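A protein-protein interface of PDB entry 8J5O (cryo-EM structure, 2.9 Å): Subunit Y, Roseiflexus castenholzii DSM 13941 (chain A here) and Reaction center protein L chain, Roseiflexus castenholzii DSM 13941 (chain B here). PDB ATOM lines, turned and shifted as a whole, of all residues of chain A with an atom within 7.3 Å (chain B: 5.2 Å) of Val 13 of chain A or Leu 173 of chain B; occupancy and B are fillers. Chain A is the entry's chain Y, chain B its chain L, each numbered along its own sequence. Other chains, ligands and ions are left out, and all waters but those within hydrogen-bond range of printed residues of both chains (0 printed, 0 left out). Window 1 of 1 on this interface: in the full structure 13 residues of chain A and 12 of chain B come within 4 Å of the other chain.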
ATOM      1  N   VAL A   5     -11.291  14.830  -1.195  1.00  0.00           N
ATOM      2  CA  VAL A   5     -11.784  16.175  -1.476  1.00  0.00           C
ATOM      3  C   VAL A   5     -11.045  16.781  -2.663  1.00  0.00           C
ATOM      4  O   VAL A   5     -11.648  17.455  -3.509  1.00  0.00           O
ATOM      5  CB  VAL A   5     -11.666  17.056  -0.219  1.00  0.00           C
ATOM      6  CG1 VAL A   5     -12.105  18.479  -0.526  1.00  0.00           C
ATOM      7  CG2 VAL A   5     -12.496  16.476   0.914  1.00  0.00           C
ATOM      8  N   ALA A   6      -9.731  16.560  -2.742  1.00  0.00           N
ATOM      9  CA  ALA A   6      -8.961  17.075  -3.868  1.00  0.00           C
ATOM     10  C   ALA A   6      -9.432  16.468  -5.182  1.00  0.00           C
ATOM     11  O   ALA A   6      -9.574  17.176  -6.188  1.00  0.00           O
ATOM     12  CB  ALA A   6      -7.473  16.806  -3.654  1.00  0.00           C
ATOM     13  N   THR A   7      -9.688  15.158  -5.195  1.00  0.00           N
ATOM     14  CA  THR A   7     -10.176  14.521  -6.412  1.00  0.00           C
ATOM     15  C   THR A   7     -11.574  15.012  -6.769  1.00  0.00           C
ATOM     16  O   THR A   7     -11.902  15.166  -7.950  1.00  0.00           O
ATOM     17  CB  THR A   7     -10.155  13.003  -6.255  1.00  0.00           C
ATOM     18  OG1 THR A   7      -8.797  12.548  -6.225  1.00  0.00           O
ATOM     19  CG2 THR A   7     -10.868  12.342  -7.420  1.00  0.00           C
ATOM     20  N   PHE A   8     -12.412  15.275  -5.762  1.00  0.00           N
ATOM     21  CA  PHE A   8     -13.730  15.842  -6.029  1.00  0.00           C
ATOM     22  C   PHE A   8     -13.623  17.210  -6.693  1.00  0.00           C
ATOM     23  O   PHE A   8     -14.295  17.478  -7.698  1.00  0.00           O
ATOM     24  CB  PHE A   8     -14.527  15.941  -4.729  1.00  0.00           C
ATOM     25  CG  PHE A   8     -15.404  14.754  -4.464  1.00  0.00           C
ATOM     26  CD1 PHE A   8     -16.480  14.475  -5.287  1.00  0.00           C
ATOM     27  CD2 PHE A   8     -15.156  13.920  -3.386  1.00  0.00           C
ATOM     28  CE1 PHE A   8     -17.292  13.384  -5.044  1.00  0.00           C
ATOM     29  CE2 PHE A   8     -15.964  12.826  -3.138  1.00  0.00           C
ATOM     30  CZ  PHE A   8     -17.033  12.558  -3.968  1.00  0.00           C
ATOM     31  N   MET A   9     -12.771  18.087  -6.155  1.00  0.00           N
ATOM     32  CA  MET A   9     -12.606  19.413  -6.749  1.00  0.00           C
ATOM     33  C   MET A   9     -12.030  19.321  -8.160  1.00  0.00           C
ATOM     34  O   MET A   9     -12.424  20.084  -9.054  1.00  0.00           O
ATOM     35  CB  MET A   9     -11.721  20.285  -5.858  1.00  0.00           C
ATOM     36  CG  MET A   9     -12.062  20.243  -4.378  1.00  0.00           C
ATOM     37  SD  MET A   9     -13.449  21.302  -3.926  1.00  0.00           S
ATOM     38  CE  MET A   9     -14.791  20.121  -3.874  1.00  0.00           C
ATOM     39  N   LEU A  10     -11.096  18.393  -8.379  1.00  0.00           N
ATOM     40  CA  LEU A  10     -10.589  18.169  -9.729  1.00  0.00           C
ATOM     41  C   LEU A  10     -11.708  17.739 -10.667  1.00  0.00           C
ATOM     42  O   LEU A  10     -11.765  18.179 -11.823  1.00  0.00           O
ATOM     43  CB  LEU A  10      -9.473  17.125  -9.701  1.00  0.00           C
ATOM     44  CG  LEU A  10      -8.660  16.939 -10.982  1.00  0.00           C
ATOM     45  CD1 LEU A  10      -7.849  18.183 -11.294  1.00  0.00           C
ATOM     46  CD2 LEU A  10      -7.754  15.726 -10.857  1.00  0.00           C
ATOM     47  N   MET A  11     -12.608  16.879 -10.188  1.00  0.00           N
ATOM     48  CA  MET A  11     -13.745  16.471 -11.004  1.00  0.00           C
ATOM     49  C   MET A  11     -14.632  17.660 -11.345  1.00  0.00           C
ATOM     50  O   MET A  11     -15.138  17.759 -12.466  1.00  0.00           O
ATOM     51  CB  MET A  11     -14.546  15.387 -10.287  1.00  0.00           C
ATOM     52  CG  MET A  11     -13.929  14.006 -10.392  1.00  0.00           C
ATOM     53  SD  MET A  11     -13.262  13.675 -12.035  1.00  0.00           S
ATOM     54  CE  MET A  11     -14.723  13.891 -13.049  1.00  0.00           C
ATOM     55  N   PHE A  12     -14.830  18.574 -10.393  1.00  0.00           N
ATOM     56  CA  PHE A  12     -15.601  19.782 -10.696  1.00  0.00           C
ATOM     57  C   PHE A  12     -14.923  20.626 -11.774  1.00  0.00           C
ATOM     58  O   PHE A  12     -15.595  21.182 -12.651  1.00  0.00           O
ATOM     59  CB  PHE A  12     -15.841  20.619  -9.437  1.00  0.00           C
ATOM     60  CG  PHE A  12     -16.935  20.091  -8.545  1.00  0.00           C
ATOM     61  CD1 PHE A  12     -18.238  20.529  -8.701  1.00  0.00           C
ATOM     62  CD2 PHE A  12     -16.661  19.194  -7.532  1.00  0.00           C
ATOM     63  CE1 PHE A  12     -19.247  20.057  -7.882  1.00  0.00           C
ATOM     64  CE2 PHE A  12     -17.663  18.719  -6.710  1.00  0.00           C
ATOM     65  CZ  PHE A  12     -18.956  19.153  -6.884  1.00  0.00           C
ATOM     66  N   VAL A  13     -13.595  20.743 -11.724  1.00  0.00           N
ATOM     67  CA  VAL A  13     -12.889  21.522 -12.745  1.00  0.00           C
ATOM     68  C   VAL A  13     -13.045  20.878 -14.125  1.00  0.00           C
ATOM     69  O   VAL A  13     -13.339  21.553 -15.127  1.00  0.00           O
ATOM     70  CB  VAL A  13     -11.408  21.693 -12.362  1.00  0.00           C
ATOM     71  CG1 VAL A  13     -10.741  22.712 -13.268  1.00  0.00           C
ATOM     72  CG2 VAL A  13     -11.287  22.123 -10.913  1.00  0.00           C
ATOM     73  N   LEU A  14     -12.848  19.560 -14.201  1.00  0.00           N
ATOM     74  CA  LEU A  14     -13.044  18.870 -15.475  1.00  0.00           C
ATOM     75  C   LEU A  14     -14.491  18.942 -15.951  1.00  0.00           C
ATOM     76  O   LEU A  14     -14.740  18.924 -17.161  1.00  0.00           O
ATOM     77  CB  LEU A  14     -12.565  17.420 -15.386  1.00  0.00           C
ATOM     78  CG  LEU A  14     -11.050  17.193 -15.475  1.00  0.00           C
ATOM     79  CD1 LEU A  14     -10.296  17.649 -14.253  1.00  0.00           C
ATOM     80  CD2 LEU A  14     -10.769  15.724 -15.739  1.00  0.00           C
ATOM     81  N   VAL A  15     -15.453  19.019 -15.032  1.00  0.00           N
ATOM     82  CA  VAL A  15     -16.833  19.279 -15.433  1.00  0.00           C
ATOM     83  C   VAL A  15     -16.950  20.666 -16.050  1.00  0.00           C
ATOM     84  O   VAL A  15     -17.642  20.859 -17.056  1.00  0.00           O
ATOM     85  CB  VAL A  15     -17.789  19.109 -14.238  1.00  0.00           C
ATOM     86  CG1 VAL A  15     -19.190  19.530 -14.627  1.00  0.00           C
ATOM     87  CG2 VAL A  15     -17.794  17.666 -13.763  1.00  0.00           C
ATOM     88  N   ALA A  16     -16.281  21.654 -15.448  1.00  0.00           N
ATOM     89  CA  ALA A  16     -16.317  23.015 -15.980  1.00  0.00           C
ATOM     90  C   ALA A  16     -15.760  23.083 -17.395  1.00  0.00           C
ATOM     91  O   ALA A  16     -16.192  23.924 -18.191  1.00  0.00           O
ATOM     92  CB  ALA A  16     -15.544  23.961 -15.063  1.00  0.00           C
ATOM     93  N   PHE A  17     -14.796  22.220 -17.724  1.00  0.00           N
ATOM     94  CA  PHE A  17     -14.342  22.135 -19.118  1.00  0.00           C
ATOM     95  C   PHE A  17     -15.440  21.721 -20.098  1.00  0.00           C
ATOM     96  O   PHE A  17     -15.306  21.980 -21.299  1.00  0.00           O
ATOM     97  CB  PHE A  17     -13.177  21.154 -19.283  1.00  0.00           C
ATOM     98  CG  PHE A  17     -11.897  21.586 -18.630  1.00  0.00           C
ATOM     99  CD1 PHE A  17     -11.069  22.496 -19.260  1.00  0.00           C
ATOM    100  CD2 PHE A  17     -11.497  21.054 -17.422  1.00  0.00           C
ATOM    101  CE1 PHE A  17      -9.880  22.888 -18.681  1.00  0.00           C
ATOM    102  CE2 PHE A  17     -10.311  21.445 -16.835  1.00  0.00           C
ATOM    103  CZ  PHE A  17      -9.502  22.362 -17.467  1.00  0.00           C
ATOM    104  N   LEU A  18     -16.513  21.083 -19.628  1.00  0.00           N
ATOM    105  CA  LEU A  18     -17.422  20.369 -20.526  1.00  0.00           C
ATOM    106  C   LEU A  18     -18.163  21.242 -21.538  1.00  0.00           C
ATOM    107  O   LEU A  18     -18.265  20.828 -22.706  1.00  0.00           O
ATOM    108  CB  LEU A  18     -18.414  19.547 -19.695  1.00  0.00           C
ATOM    109  CG  LEU A  18     -19.383  18.695 -20.517  1.00  0.00           C
ATOM    110  CD1 LEU A  18     -18.618  17.663 -21.323  1.00  0.00           C
ATOM    111  CD2 LEU A  18     -20.392  18.010 -19.622  1.00  0.00           C
ATOM    112  N   ILE B 168     -14.447  30.786  -9.468  1.00  0.00           N
ATOM    113  CA  ILE B 168     -14.806  29.814  -8.438  1.00  0.00           C
ATOM    114  C   ILE B 168     -13.636  28.901  -8.106  1.00  0.00           C
ATOM    115  O   ILE B 168     -13.476  28.487  -6.952  1.00  0.00           O
ATOM    116  CB  ILE B 168     -16.047  29.004  -8.859  1.00  0.00           C
ATOM    117  CG1 ILE B 168     -17.264  29.919  -9.002  1.00  0.00           C
ATOM    118  CG2 ILE B 168     -16.324  27.889  -7.864  1.00  0.00           C
ATOM    119  CD1 ILE B 168     -18.455  29.255  -9.655  1.00  0.00           C
ATOM    120  N   THR B 169     -12.810  28.557  -9.097  1.00  0.00           N
ATOM    121  CA  THR B 169     -11.625  27.753  -8.819  1.00  0.00           C
ATOM    122  C   THR B 169     -10.687  28.468  -7.855  1.00  0.00           C
ATOM    123  O   THR B 169     -10.182  27.863  -6.903  1.00  0.00           O
ATOM    124  CB  THR B 169     -10.892  27.425 -10.120  1.00  0.00           C
ATOM    125  OG1 THR B 169     -11.760  26.686 -10.987  1.00  0.00           O
ATOM    126  CG2 THR B 169      -9.643  26.611  -9.840  1.00  0.00           C
ATOM    127  N   GLN B 171     -11.352  31.029  -5.709  1.00  0.00           N
ATOM    128  CA  GLN B 171     -11.863  31.454  -4.411  1.00  0.00           C
ATOM    129  C   GLN B 171     -12.608  30.386  -3.621  1.00  0.00           C
ATOM    130  O   GLN B 171     -12.816  30.579  -2.420  1.00  0.00           O
ATOM    131  CB  GLN B 171     -12.779  32.677  -4.570  1.00  0.00           C
ATOM    132  CG  GLN B 171     -12.069  33.912  -5.095  1.00  0.00           C
ATOM    133  CD  GLN B 171     -11.293  34.647  -4.019  1.00  0.00           C
ATOM    134  OE1 GLN B 171     -10.757  34.036  -3.099  1.00  0.00           O
ATOM    135  NE2 GLN B 171     -11.230  35.965  -4.132  1.00  0.00           N
ATOM    136  N   TRP B 172     -13.024  29.281  -4.240  1.00  0.00           N
ATOM    137  CA  TRP B 172     -13.733  28.235  -3.505  1.00  0.00           C
ATOM    138  C   TRP B 172     -13.006  26.897  -3.517  1.00  0.00           C
ATOM    139  O   TRP B 172     -12.743  26.341  -2.447  1.00  0.00           O
ATOM    140  CB  TRP B 172     -15.156  28.068  -4.054  1.00  0.00           C
ATOM    141  CG  TRP B 172     -16.002  29.294  -3.938  1.00  0.00           C
ATOM    142  CD1 TRP B 172     -16.000  30.376  -4.766  1.00  0.00           C
ATOM    143  CD2 TRP B 172     -16.977  29.564  -2.928  1.00  0.00           C
ATOM    144  NE1 TRP B 172     -16.914  31.303  -4.335  1.00  0.00           N
ATOM    145  CE2 TRP B 172     -17.527  30.828  -3.206  1.00  0.00           C
ATOM    146  CE3 TRP B 172     -17.438  28.859  -1.813  1.00  0.00           C
ATOM    147  CZ2 TRP B 172     -18.520  31.400  -2.415  1.00  0.00           C
ATOM    148  CZ3 TRP B 172     -18.419  29.430  -1.026  1.00  0.00           C
ATOM    149  CH2 TRP B 172     -18.949  30.688  -1.330  1.00  0.00           C
ATOM    150  N   LEU B 173     -12.669  26.360  -4.690  1.00  0.00           N
ATOM    151  CA  LEU B 173     -12.216  24.973  -4.768  1.00  0.00           C
ATOM    152  C   LEU B 173     -10.827  24.798  -4.164  1.00  0.00           C
ATOM    153  O   LEU B 173     -10.593  23.864  -3.390  1.00  0.00           O
ATOM    154  CB  LEU B 173     -12.237  24.497  -6.218  1.00  0.00           C
ATOM    155  CG  LEU B 173     -13.563  24.642  -6.966  1.00  0.00           C
ATOM    156  CD1 LEU B 173     -13.569  23.775  -8.207  1.00  0.00           C
ATOM    157  CD2 LEU B 173     -14.736  24.294  -6.067  1.00  0.00           C
ATOM    158  N   ARG B 174      -9.888  25.672  -4.521  1.00  0.00           N
ATOM    159  CA  ARG B 174      -8.527  25.549  -4.001  1.00  0.00           C
ATOM    160  C   ARG B 174      -8.459  25.707  -2.488  1.00  0.00           C
ATOM    161  O   ARG B 174      -7.811  24.873  -1.831  1.00  0.00           O
ATOM    162  CB  ARG B 174      -7.617  26.556  -4.709  1.00  0.00           C
ATOM    163  CG  ARG B 174      -6.134  26.231  -4.631  1.00  0.00           C
ATOM    164  CD  ARG B 174      -5.336  27.114  -5.571  1.00  0.00           C
ATOM    165  NE  ARG B 174      -3.897  26.957  -5.403  1.00  0.00           N
ATOM    166  CZ  ARG B 174      -3.185  27.523  -4.437  1.00  0.00           C
ATOM    167  NH1 ARG B 174      -3.750  28.292  -3.522  1.00  0.00           N
ATOM    168  NH2 ARG B 174      -1.873  27.317  -4.393  1.00  0.00           N
ATOM    169  N   PRO B 175      -9.060  26.734  -1.875  1.00  0.00           N
ATOM    170  CA  PRO B 175      -9.034  26.818  -0.405  1.00  0.00           C
ATOM    171  C   PRO B 175      -9.663  25.626   0.296  1.00  0.00           C
ATOM    172  O   PRO B 175      -9.175  25.217   1.356  1.00  0.00           O
ATOM    173  CB  PRO B 175      -9.805  28.114  -0.122  1.00  0.00           C
ATOM    174  CG  PRO B 175      -9.620  28.928  -1.343  1.00  0.00           C
ATOM    175  CD  PRO B 175      -9.589  27.966  -2.486  1.00  0.00           C
ATOM    176  N   ILE B 176     -10.739  25.060  -0.255  1.00  0.00           N
ATOM    177  CA  ILE B 176     -11.362  23.898   0.374  1.00  0.00           C
ATOM    178  C   ILE B 176     -10.478  22.667   0.229  1.00  0.00           C
ATOM    179  O   ILE B 176     -10.318  21.890   1.177  1.00  0.00           O
ATOM    180  CB  ILE B 176     -12.768  23.654  -0.205  1.00  0.00           C
ATOM    181  CG1 ILE B 176     -13.687  24.836   0.105  1.00  0.00           C
ATOM    182  CG2 ILE B 176     -13.352  22.366   0.342  1.00  0.00           C
ATOM    183  CD1 ILE B 176     -14.999  24.798  -0.640  1.00  0.00           C
ATOM    184  N   ALA B 177      -9.900  22.462  -0.956  1.00  0.00           N
ATOM    185  CA  ALA B 177      -9.033  21.308  -1.165  1.00  0.00           C
ATOM    186  C   ALA B 177      -7.796  21.378  -0.279  1.00  0.00           C
ATOM    187  O   ALA B 177      -7.371  20.364   0.285  1.00  0.00           O
ATOM    188  CB  ALA B 177      -8.638  21.204  -2.637  1.00  0.00           C
ATOM    189  N   MET B 178      -7.202  22.565  -0.145  1.00  0.00           N
ATOM    190  CA  MET B 178      -6.066  22.728   0.755  1.00  0.00           C
ATOM    191  C   MET B 178      -6.486  22.787   2.218  1.00  0.00           C
ATOM    192  O   MET B 178      -5.647  22.571   3.099  1.00  0.00           O
ATOM    193  CB  MET B 178      -5.271  23.977   0.371  1.00  0.00           C
ATOM    194  CG  MET B 178      -5.019  24.088  -1.125  1.00  0.00           C
ATOM    195  SD  MET B 178      -3.690  25.212  -1.582  1.00  0.00           S
ATOM    196  CE  MET B 178      -2.372  24.632  -0.524  1.00  0.00           C
ATOM    197  N   ASN B 279      -7.246  27.931 -15.310  1.00  0.00           N
ATOM    198  CA  ASN B 279      -7.777  27.494 -14.022  1.00  0.00           C
ATOM    199  C   ASN B 279      -7.335  26.069 -13.701  1.00  0.00           C
ATOM    200  O   ASN B 279      -7.077  25.745 -12.530  1.00  0.00           O
ATOM    201  CB  ASN B 279      -9.304  27.695 -13.965  1.00  0.00           C
ATOM    202  CG  ASN B 279     -10.108  26.720 -14.828  1.00  0.00           C
ATOM    203  OD1 ASN B 279      -9.770  25.551 -15.004  1.00  0.00           O
ATOM    204  ND2 ASN B 279     -11.222  27.219 -15.351  1.00  0.00           N
ATOM    205  N   LEU B 280      -7.193  25.226 -14.728  1.00  0.00           N
ATOM    206  CA  LEU B 280      -6.662  23.887 -14.505  1.00  0.00           C
ATOM    207  C   LEU B 280      -5.252  23.939 -13.923  1.00  0.00           C
ATOM    208  O   LEU B 280      -4.938  23.217 -12.967  1.00  0.00           O
ATOM    209  CB  LEU B 280      -6.678  23.092 -15.810  1.00  0.00           C
ATOM    210  CG  LEU B 280      -6.210  21.638 -15.733  1.00  0.00           C
ATOM    211  CD1 LEU B 280      -7.118  20.833 -14.827  1.00  0.00           C
ATOM    212  CD2 LEU B 280      -6.170  21.028 -17.120  1.00  0.00           C
ATOM    213  N   PHE B 283      -5.254  25.185 -10.180  1.00  0.00           N
ATOM    214  CA  PHE B 283      -5.719  24.185  -9.224  1.00  0.00           C
ATOM    215  C   PHE B 283      -4.704  23.058  -9.081  1.00  0.00           C
ATOM    216  O   PHE B 283      -4.441  22.593  -7.966  1.00  0.00           O
ATOM    217  CB  PHE B 283      -7.107  23.657  -9.622  1.00  0.00           C
ATOM    218  CG  PHE B 283      -7.649  22.570  -8.706  1.00  0.00           C
ATOM    219  CD1 PHE B 283      -7.253  21.238  -8.822  1.00  0.00           C
ATOM    220  CD2 PHE B 283      -8.514  22.907  -7.681  1.00  0.00           C
ATOM    221  CE1 PHE B 283      -7.739  20.278  -7.965  1.00  0.00           C
ATOM    222  CE2 PHE B 283      -9.000  21.946  -6.823  1.00  0.00           C
ATOM    223  CZ  PHE B 283      -8.609  20.631  -6.965  1.00  0.00           C
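Of the 14 printed residues of chain A, 5 touch a printed residue of chain B.
Printed residues of chain A that touch a printed residue of chain B: Ala 6, Met 9, Leu 10, Val 13 and Phe 17.
Of the 13 printed residues of chain B, 5 touch a printed residue of chain A.
Printed residues of chain B that touch a printed residue of chain A: Leu 173, Ala 177, Asn 279, Leu 280 and Phe 283.
Hydrophobic or aromatic side chains of chain B within 4 Å of the printed part of chain A: Leu 173, Ala 177, Leu 280 and Phe 283.
Among the printed residues, 8 pairs touch across the chains.
Among the printed residues, no Asp or Glu carboxylate lies within 4 Å of a Lys or Arg side-chain nitrogen of the other chain.
O of Ala 6 of chain A touches CZ of Phe 283 of chain B, 3.7 Å away.
SD of Met 9 of chain A touches O of Leu 173 of chain B, at 3.9 Å.
CB of Ala 177 of chain B touches CG of Met 9 of chain A, at 3.96 Å.
CZ of Phe 283 of chain B touches CB of Met 9 of chain A, at 3.3 Å.
Phe 283 of chain B touches Leu 10 of chain A.
Leu 173 of chain B touches Val 13 of chain A.
OD1 of Asn 279 of chain B touches CG1 of Val 13 of chain A (3.5 Å).
Leu 280 of chain B touches Phe 17 of chain A (CB to CZ, 3.4 Å).
Of the printed residues of chain B, Leu 10 of chain A touches Phe 283.
Met 11 of chain A touches none of the printed residues of chain B.
Leu 14 of chain A touches none of the printed residues of chain B.
Printed residues of chain B within 4 Å of Phe 17 of chain A: Leu 280 (3.4 Å).
Of chain A, only Met 9 and Val 13 come within 4 Å of Leu 173 of chain B.
Of the printed residues of chain A, Leu 280 of chain B touches Phe 17.
The nearest residue of chain B that does not touch Val 13 of chain A is Phe 283 of chain B (4.3 Å).
The nearest residue of chain A that does not touch Leu 173 of chain B is Phe 12 of chain A (4.1 Å).
The backbone NH (N) of Leu 173 of chain B is in hydrogen-bond range of the backbone carbonyl oxygen (O) of Ile 168 of chain B (3.2 Å).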
